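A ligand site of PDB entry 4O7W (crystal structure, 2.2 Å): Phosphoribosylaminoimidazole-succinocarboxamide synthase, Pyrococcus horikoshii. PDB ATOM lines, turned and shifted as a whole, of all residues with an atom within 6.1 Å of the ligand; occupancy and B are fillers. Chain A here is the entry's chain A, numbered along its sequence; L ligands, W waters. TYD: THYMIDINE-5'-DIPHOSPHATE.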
ATOM      1  N   GLU A  89     -23.917   4.501   2.542  1.00  0.00           N
ATOM      2  CA  GLU A  89     -22.550   4.976   2.661  1.00  0.00           C
ATOM      3  C   GLU A  89     -22.019   4.279   3.896  1.00  0.00           C
ATOM      4  O   GLU A  89     -22.606   4.382   4.973  1.00  0.00           O
ATOM      5  CB  GLU A  89     -22.541   6.502   2.757  1.00  0.00           C
ATOM      6  CG  GLU A  89     -22.779   7.132   1.375  1.00  0.00           C
ATOM      7  CD  GLU A  89     -23.367   8.535   1.435  1.00  0.00           C
ATOM      8  OE1 GLU A  89     -23.490   9.155   0.346  1.00  0.00           O
ATOM      9  OE2 GLU A  89     -23.719   9.013   2.549  1.00  0.00           O
ATOM     10  N   VAL A  91     -19.154   3.818   6.528  1.00  0.00           N
ATOM     11  CA  VAL A  91     -18.062   4.605   7.082  1.00  0.00           C
ATOM     12  C   VAL A  91     -17.244   3.767   8.088  1.00  0.00           C
ATOM     13  O   VAL A  91     -17.812   3.155   9.006  1.00  0.00           O
ATOM     14  CB  VAL A  91     -18.583   5.924   7.702  1.00  0.00           C
ATOM     15  CG1 VAL A  91     -17.437   6.675   8.362  1.00  0.00           C
ATOM     16  CG2 VAL A  91     -19.256   6.811   6.637  1.00  0.00           C
ATOM     17  N   VAL A  92     -15.932   3.712   7.889  1.00  0.00           N
ATOM     18  CA  VAL A  92     -15.027   3.042   8.808  1.00  0.00           C
ATOM     19  C   VAL A  92     -14.152   4.115   9.477  1.00  0.00           C
ATOM     20  O   VAL A  92     -13.686   5.030   8.815  1.00  0.00           O
ATOM     21  CB  VAL A  92     -14.112   2.025   8.058  1.00  0.00           C
ATOM     22  CG1 VAL A  92     -13.249   1.245   9.031  1.00  0.00           C
ATOM     23  CG2 VAL A  92     -14.951   1.076   7.206  1.00  0.00           C
ATOM     24  N   ARG A  93     -13.981   4.021  10.796  1.00  0.00           N
ATOM     25  CA  ARG A  93     -13.306   5.067  11.567  1.00  0.00           C
ATOM     26  C   ARG A  93     -12.245   4.449  12.508  1.00  0.00           C
ATOM     27  O   ARG A  93     -12.546   3.540  13.277  1.00  0.00           O
ATOM     28  CB  ARG A  93     -14.338   5.908  12.348  1.00  0.00           C
ATOM     29  CG  ARG A  93     -15.712   6.029  11.656  1.00  0.00           C
ATOM     30  CD  ARG A  93     -16.697   6.980  12.343  1.00  0.00           C
ATOM     31  NE  ARG A  93     -16.283   8.366  12.160  1.00  0.00           N
ATOM     32  CZ  ARG A  93     -16.979   9.332  11.574  1.00  0.00           C
ATOM     33  NH1 ARG A  93     -18.221   9.149  11.101  1.00  0.00           N
ATOM     34  NH2 ARG A  93     -16.416  10.515  11.460  1.00  0.00           N
ATOM     35  N   ALA A  97     -12.882  11.907  14.581  1.00  0.00           N
ATOM     36  CA  ALA A  97     -12.922  13.134  13.782  1.00  0.00           C
ATOM     37  C   ALA A  97     -14.340  13.301  13.258  1.00  0.00           C
ATOM     38  O   ALA A  97     -15.159  12.382  13.352  1.00  0.00           O
ATOM     39  CB  ALA A  97     -11.924  13.051  12.630  1.00  0.00           C
ATOM     40  N   GLY A  98     -14.605  14.478  12.691  1.00  0.00           N
ATOM     41  CA  GLY A  98     -15.889  14.772  12.065  1.00  0.00           C
ATOM     42  C   GLY A  98     -17.087  14.512  12.970  1.00  0.00           C
ATOM     43  O   GLY A  98     -17.079  14.871  14.153  1.00  0.00           O
ATOM     44  N   SER A  99     -18.092  13.854  12.402  1.00  0.00           N
ATOM     45  CA  SER A  99     -19.380  13.650  13.092  1.00  0.00           C
ATOM     46  C   SER A  99     -19.296  12.729  14.301  1.00  0.00           C
ATOM     47  O   SER A  99     -20.171  12.778  15.166  1.00  0.00           O
ATOM     48  CB  SER A  99     -20.420  13.086  12.097  1.00  0.00           C
ATOM     49  OG  SER A  99     -20.140  11.718  11.854  1.00  0.00           O
ATOM     50  N   LEU A 100     -18.279  11.866  14.362  1.00  0.00           N
ATOM     51  CA  LEU A 100     -18.112  10.991  15.531  1.00  0.00           C
ATOM     52  C   LEU A 100     -18.010  11.771  16.859  1.00  0.00           C
ATOM     53  O   LEU A 100     -18.359  11.248  17.921  1.00  0.00           O
ATOM     54  CB  LEU A 100     -16.920  10.034  15.344  1.00  0.00           C
ATOM     55  CG  LEU A 100     -16.803   8.921  16.383  1.00  0.00           C
ATOM     56  CD1 LEU A 100     -18.046   8.037  16.420  1.00  0.00           C
ATOM     57  CD2 LEU A 100     -15.544   8.080  16.185  1.00  0.00           C
ATOM     58  N   GLU A 118     -19.982   2.519  10.531  1.00  0.00           N
ATOM     59  CA  GLU A 118     -21.278   3.185  10.587  1.00  0.00           C
ATOM     60  C   GLU A 118     -21.946   3.065   9.223  1.00  0.00           C
ATOM     61  O   GLU A 118     -21.293   3.170   8.173  1.00  0.00           O
ATOM     62  CB  GLU A 118     -21.131   4.654  10.970  1.00  0.00           C
ATOM     63  CG  GLU A 118     -20.492   4.912  12.331  1.00  0.00           C
ATOM     64  CD  GLU A 118     -20.169   6.382  12.578  1.00  0.00           C
ATOM     65  OE1 GLU A 118     -20.132   7.171  11.603  1.00  0.00           O
ATOM     66  OE2 GLU A 118     -19.948   6.763  13.738  1.00  0.00           O
ATOM     67  N   TYR A 120     -24.860   4.634   6.782  1.00  0.00           N
ATOM     68  CA  TYR A 120     -25.683   5.807   6.512  1.00  0.00           C
ATOM     69  C   TYR A 120     -26.570   5.494   5.332  1.00  0.00           C
ATOM     70  O   TYR A 120     -26.108   5.010   4.304  1.00  0.00           O
ATOM     71  CB  TYR A 120     -24.817   7.038   6.218  1.00  0.00           C
ATOM     72  CG  TYR A 120     -24.070   7.537   7.428  1.00  0.00           C
ATOM     73  CD1 TYR A 120     -24.665   8.440   8.319  1.00  0.00           C
ATOM     74  CD2 TYR A 120     -22.787   7.071   7.711  1.00  0.00           C
ATOM     75  CE1 TYR A 120     -23.992   8.882   9.444  1.00  0.00           C
ATOM     76  CE2 TYR A 120     -22.096   7.505   8.821  1.00  0.00           C
ATOM     77  CZ  TYR A 120     -22.704   8.395   9.696  1.00  0.00           C
ATOM     78  OH  TYR A 120     -21.994   8.803  10.801  1.00  0.00           O
ATOM     79  N   ASP A 128     -29.338  11.709   4.539  1.00  0.00           N
ATOM     80  CA  ASP A 128     -28.424  10.596   4.826  1.00  0.00           C
ATOM     81  C   ASP A 128     -28.278  10.226   6.325  1.00  0.00           C
ATOM     82  O   ASP A 128     -27.181  10.279   6.875  1.00  0.00           O
ATOM     83  CB  ASP A 128     -27.040  10.893   4.232  1.00  0.00           C
ATOM     84  CG  ASP A 128     -27.052  10.973   2.716  1.00  0.00           C
ATOM     85  OD1 ASP A 128     -28.132  10.982   2.091  1.00  0.00           O
ATOM     86  OD2 ASP A 128     -25.956  11.017   2.126  1.00  0.00           O
ATOM     87  N   ASP A 173     -10.408   8.056   8.893  1.00  0.00           N
ATOM     88  CA  ASP A 173     -11.699   7.419   8.590  1.00  0.00           C
ATOM     89  C   ASP A 173     -11.911   7.520   7.094  1.00  0.00           C
ATOM     90  O   ASP A 173     -11.111   8.155   6.409  1.00  0.00           O
ATOM     91  CB  ASP A 173     -12.855   8.092   9.357  1.00  0.00           C
ATOM     92  CG  ASP A 173     -12.979   9.580   9.066  1.00  0.00           C
ATOM     93  OD1 ASP A 173     -12.644  10.007   7.951  1.00  0.00           O
ATOM     94  OD2 ASP A 173     -13.445  10.314   9.944  1.00  0.00           O
ATOM     95  N   PHE A 174     -12.982   6.902   6.589  1.00  0.00           N
ATOM     96  CA  PHE A 174     -13.283   6.936   5.162  1.00  0.00           C
ATOM     97  C   PHE A 174     -14.654   6.344   4.895  1.00  0.00           C
ATOM     98  O   PHE A 174     -15.218   5.639   5.744  1.00  0.00           O
ATOM     99  CB  PHE A 174     -12.214   6.182   4.324  1.00  0.00           C
ATOM    100  CG  PHE A 174     -12.093   4.704   4.647  1.00  0.00           C
ATOM    101  CD1 PHE A 174     -12.732   3.748   3.874  1.00  0.00           C
ATOM    102  CD2 PHE A 174     -11.315   4.278   5.724  1.00  0.00           C
ATOM    103  CE1 PHE A 174     -12.614   2.391   4.138  1.00  0.00           C
ATOM    104  CE2 PHE A 174     -11.193   2.912   6.011  1.00  0.00           C
ATOM    105  CZ  PHE A 174     -11.850   1.972   5.220  1.00  0.00           C
ATOM    106  N   LYS A 175     -15.170   6.596   3.696  1.00  0.00           N
ATOM    107  CA  LYS A 175     -16.489   6.144   3.308  1.00  0.00           C
ATOM    108  C   LYS A 175     -16.385   5.264   2.043  1.00  0.00           C
ATOM    109  O   LYS A 175     -15.686   5.617   1.099  1.00  0.00           O
ATOM    110  CB  LYS A 175     -17.407   7.339   3.045  1.00  0.00           C
ATOM    111  CG  LYS A 175     -18.853   6.973   2.654  1.00  0.00           C
ATOM    112  CD  LYS A 175     -19.031   6.837   1.147  1.00  0.00           C
ATOM    113  CE  LYS A 175     -18.976   8.197   0.424  1.00  0.00           C
ATOM    114  NZ  LYS A 175     -18.783   8.024  -1.057  1.00  0.00           N
ATOM    115  N   ASP A 195     -11.317  13.122  -1.157  1.00  0.00           N
ATOM    116  CA  ASP A 195     -12.714  13.558  -0.948  1.00  0.00           C
ATOM    117  C   ASP A 195     -13.477  12.642   0.016  1.00  0.00           C
ATOM    118  O   ASP A 195     -14.375  13.101   0.721  1.00  0.00           O
ATOM    119  CB  ASP A 195     -13.506  13.577  -2.267  1.00  0.00           C
ATOM    120  CG  ASP A 195     -13.394  14.898  -3.002  1.00  0.00           C
ATOM    121  OD1 ASP A 195     -14.268  15.178  -3.845  1.00  0.00           O
ATOM    122  OD2 ASP A 195     -12.439  15.660  -2.750  1.00  0.00           O
ATOM    123  N   THR A 196     -13.141  11.353   0.003  1.00  0.00           N
ATOM    124  CA  THR A 196     -13.958  10.357   0.705  1.00  0.00           C
ATOM    125  C   THR A 196     -13.223   9.690   1.882  1.00  0.00           C
ATOM    126  O   THR A 196     -13.732   8.724   2.459  1.00  0.00           O
ATOM    127  CB  THR A 196     -14.550   9.323  -0.280  1.00  0.00           C
ATOM    128  OG1 THR A 196     -13.487   8.634  -0.944  1.00  0.00           O
ATOM    129  CG2 THR A 196     -15.433  10.015  -1.319  1.00  0.00           C
ATOM    130  N   CYS A 197     -12.043  10.215   2.220  1.00  0.00           N
ATOM    131  CA  CYS A 197     -11.213   9.708   3.324  1.00  0.00           C
ATOM    132  C   CYS A 197     -10.633  10.857   4.139  1.00  0.00           C
ATOM    133  O   CYS A 197     -10.457  11.951   3.610  1.00  0.00           O
ATOM    134  CB  CYS A 197      -9.998   8.951   2.780  1.00  0.00           C
ATOM    135  SG  CYS A 197     -10.314   7.611   1.628  1.00  0.00           S
ATOM    136  N   ARG A 198     -10.315  10.598   5.399  1.00  0.00           N
ATOM    137  CA  ARG A 198      -9.437  11.490   6.155  1.00  0.00           C
ATOM    138  C   ARG A 198      -8.025  10.911   6.203  1.00  0.00           C
ATOM    139  O   ARG A 198      -7.815   9.771   6.644  1.00  0.00           O
ATOM    140  CB  ARG A 198      -9.957  11.798   7.559  1.00  0.00           C
ATOM    141  CG  ARG A 198     -11.116  12.798   7.558  1.00  0.00           C
ATOM    142  CD  ARG A 198     -11.533  13.270   8.947  1.00  0.00           C
ATOM    143  NE  ARG A 198     -12.552  14.326   8.841  1.00  0.00           N
ATOM    144  CZ  ARG A 198     -13.869  14.132   8.940  1.00  0.00           C
ATOM    145  NH1 ARG A 198     -14.387  12.931   9.200  1.00  0.00           N
ATOM    146  NH2 ARG A 198     -14.684  15.157   8.783  1.00  0.00           N
ATOM    147  N   LYS A 210     -10.222  16.462   2.105  1.00  0.00           N
ATOM    148  CA  LYS A 210     -11.316  17.429   1.933  1.00  0.00           C
ATOM    149  C   LYS A 210     -11.573  18.348   3.150  1.00  0.00           C
ATOM    150  O   LYS A 210     -12.248  19.371   3.027  1.00  0.00           O
ATOM    151  CB  LYS A 210     -12.582  16.672   1.549  1.00  0.00           C
ATOM    152  CG  LYS A 210     -13.681  17.504   0.916  1.00  0.00           C
ATOM    153  CD  LYS A 210     -14.771  16.603   0.335  1.00  0.00           C
ATOM    154  CE  LYS A 210     -16.089  17.344   0.268  1.00  0.00           C
ATOM    155  NZ  LYS A 210     -17.247  16.477  -0.081  1.00  0.00           N
ATOM    156  N   ASP A 211     -11.058  17.983   4.332  1.00  0.00           N
ATOM    157  CA  ASP A 211     -11.206  18.811   5.543  1.00  0.00           C
ATOM    158  C   ASP A 211     -10.532  20.199   5.343  1.00  0.00           C
ATOM    159  O   ASP A 211     -10.982  21.204   5.899  1.00  0.00           O
ATOM    160  CB  ASP A 211     -10.655  18.108   6.786  1.00  0.00           C
ATOM    161  CG  ASP A 211     -11.705  17.198   7.477  1.00  0.00           C
ATOM    162  OD1 ASP A 211     -12.918  17.239   7.166  1.00  0.00           O
ATOM    163  OD2 ASP A 211     -11.297  16.437   8.370  1.00  0.00           O
ATOM    164  N   ARG A 214     -13.365  21.877   3.735  1.00  0.00           N
ATOM    165  CA  ARG A 214     -14.478  21.993   4.693  1.00  0.00           C
ATOM    166  C   ARG A 214     -14.244  23.098   5.736  1.00  0.00           C
ATOM    167  O   ARG A 214     -15.159  23.870   6.043  1.00  0.00           O
ATOM    168  CB  ARG A 214     -14.738  20.652   5.423  1.00  0.00           C
ATOM    169  CG  ARG A 214     -15.372  19.543   4.610  1.00  0.00           C
ATOM    170  CD  ARG A 214     -15.577  18.319   5.497  1.00  0.00           C
ATOM    171  NE  ARG A 214     -16.001  17.132   4.752  1.00  0.00           N
ATOM    172  CZ  ARG A 214     -15.231  16.086   4.459  1.00  0.00           C
ATOM    173  NH1 ARG A 214     -15.741  15.077   3.776  1.00  0.00           N
ATOM    174  NH2 ARG A 214     -13.946  16.021   4.850  1.00  0.00           N
ATOM    175  N   PHE A 215     -13.034  23.154   6.276  1.00  0.00           N
ATOM    176  CA  PHE A 215     -12.716  24.074   7.374  1.00  0.00           C
ATOM    177  C   PHE A 215     -11.646  25.121   7.053  1.00  0.00           C
ATOM    178  O   PHE A 215     -11.050  25.694   7.972  1.00  0.00           O
ATOM    179  CB  PHE A 215     -12.348  23.294   8.648  1.00  0.00           C
ATOM    180  CG  PHE A 215     -13.378  22.258   9.028  1.00  0.00           C
ATOM    181  CD1 PHE A 215     -14.655  22.641   9.431  1.00  0.00           C
ATOM    182  CD2 PHE A 215     -13.074  20.899   8.967  1.00  0.00           C
ATOM    183  CE1 PHE A 215     -15.615  21.689   9.758  1.00  0.00           C
ATOM    184  CE2 PHE A 215     -14.025  19.949   9.297  1.00  0.00           C
ATOM    185  CZ  PHE A 215     -15.300  20.343   9.690  1.00  0.00           C
HETATM  186  PA  TYD L   1     -18.202  12.085   8.836  1.00  0.00           P
HETATM  187  O1A TYD L   1     -17.266  12.497   9.922  1.00  0.00           O
HETATM  188  O2A TYD L   1     -19.286  11.099   9.241  1.00  0.00           O
HETATM  189  O3A TYD L   1     -18.990  13.305   8.152  1.00  0.00           O
HETATM  190  PB  TYD L   1     -18.442  14.753   7.713  1.00  0.00           P
HETATM  191  O1B TYD L   1     -17.457  15.205   8.767  1.00  0.00           O
HETATM  192  O2B TYD L   1     -17.763  14.509   6.374  1.00  0.00           O
HETATM  193  O3B TYD L   1     -19.704  15.554   7.585  1.00  0.00           O
HETATM  194  O5' TYD L   1     -17.340  11.494   7.636  1.00  0.00           O
HETATM  195  C5' TYD L   1     -16.566  10.329   7.833  1.00  0.00           C
HETATM  196  C4' TYD L   1     -15.660  10.043   6.635  1.00  0.00           C
HETATM  197  O4' TYD L   1     -16.446   9.488   5.578  1.00  0.00           O
HETATM  198  C3' TYD L   1     -14.953  11.274   6.052  1.00  0.00           C
HETATM  199  O3' TYD L   1     -13.681  10.857   5.570  1.00  0.00           O
HETATM  200  C2' TYD L   1     -15.792  11.675   4.864  1.00  0.00           C
HETATM  201  C1' TYD L   1     -16.442  10.368   4.444  1.00  0.00           C
HETATM  202  N1  TYD L   1     -17.826  10.535   3.998  1.00  0.00           N
HETATM  203  C2  TYD L   1     -18.108  10.942   2.652  1.00  0.00           C
HETATM  204  O2  TYD L   1     -17.172  11.143   1.857  1.00  0.00           O
HETATM  205  N3  TYD L   1     -19.365  11.084   2.233  1.00  0.00           N
HETATM  206  C4  TYD L   1     -20.406  10.833   3.070  1.00  0.00           C
HETATM  207  O4  TYD L   1     -21.570  10.954   2.675  1.00  0.00           O
HETATM  208  C5  TYD L   1     -20.162  10.388   4.475  1.00  0.00           C
HETATM  209  C5M TYD L   1     -21.290  10.102   5.437  1.00  0.00           C
HETATM  210  C6  TYD L   1     -18.834  10.271   4.869  1.00  0.00           C
HETATM  211  O   HOH W   1     -12.644  13.440   3.749  1.00  0.00           O
HETATM  212  O   HOH W   2     -21.938  11.531   8.529  1.00  0.00           O
HETATM  213  O   HOH W   3     -18.461  16.709  10.873  1.00  0.00           O
HETATM  214  O   HOH W   4     -23.716  11.869   3.617  1.00  0.00           O
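The guanidinium group of Arg 198 lies within salt-bridge range of the side-chain carboxylate of Asp 211. The side-chain carboxylate of Glu 118 is in salt-bridge range of the guanidinium group of Arg 93 (2.8 Å). The backbone NH (N) of Val 92 is in hydrogen-bond range of the backbone carbonyl oxygen (O) of Phe 174. O of Val 91 lies within hydrogen-bond range of N of Glu 118, at 2.7 Å. The backbone NH (N) of Lys 175 is in hydrogen-bond range of the backbone carbonyl oxygen (O) of Thr 196 (2.9 Å). The side-chain carboxylate (OD2) of Asp 173 lies within salt-bridge range of the guanidinium group (NH2) of Arg 93, 3.3 Å away. OH of Tyr 120 sits at hydrogen-bond distance from OE1 of Glu 118 (2.6 Å). The backbone NH (N) of Glu 89 is in hydrogen-bond range of the backbone carbonyl oxygen (O) of Tyr 120 (2.9 Å).
OE2 of Glu 89 lies close to O4 of the ligand. Val 91 touches the ligand. CA of Gly 98 touches O1A of the ligand, at 3.4 Å. OH of Tyr 120 touches O2A of the ligand, 3.9 Å away. Phe 174 touches the ligand (C to O4', 3.7 Å). Lys 175 touches the ligand. Asp 195 touches the ligand (O to O2, 3.6 Å). CA of Thr 196 touches O2 of the ligand (3.5 Å). Cys 197 touches the ligand. Hydrophobic or aromatic side chains that line the ligand: Val 91.
Water W3 lies within hydrogen-bond range of O1B of the ligand and N of Ser 99. Water W1 lies within hydrogen-bond range of the backbone carbonyl oxygen (O) of Cys 197 (2.6 Å), the guanidinium group (NH2) of Arg 214 (3.1 Å) and an oxygen (O3') of the ligand (3.3 Å).
The side-chain hydroxyl (OG) of Ser 99 sits at hydrogen-bond distance from an oxygen (O2A) of the ligand (2.8 Å). N of Arg 198 lies within hydrogen-bond range of O3' of the ligand (3.4 Å). The guanidinium group (NH2) of Arg 198 is in salt-bridge range of an oxygen (O1B) of the ligand (2.8 Å). The side-chain carboxylate (OD1) of Asp 173 lies within hydrogen-bond range of an oxygen (O3') of the ligand (2.7 Å). NH2 of Arg 93 is in salt-bridge range of O1A of the ligand (2.6 Å). An oxygen (O2B) of the ligand is in salt-bridge range of the guanidinium group of Arg 214 (3.3 Å). O1A of the ligand sits at hydrogen-bond distance from N of Ser 99, 2.9 Å away.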
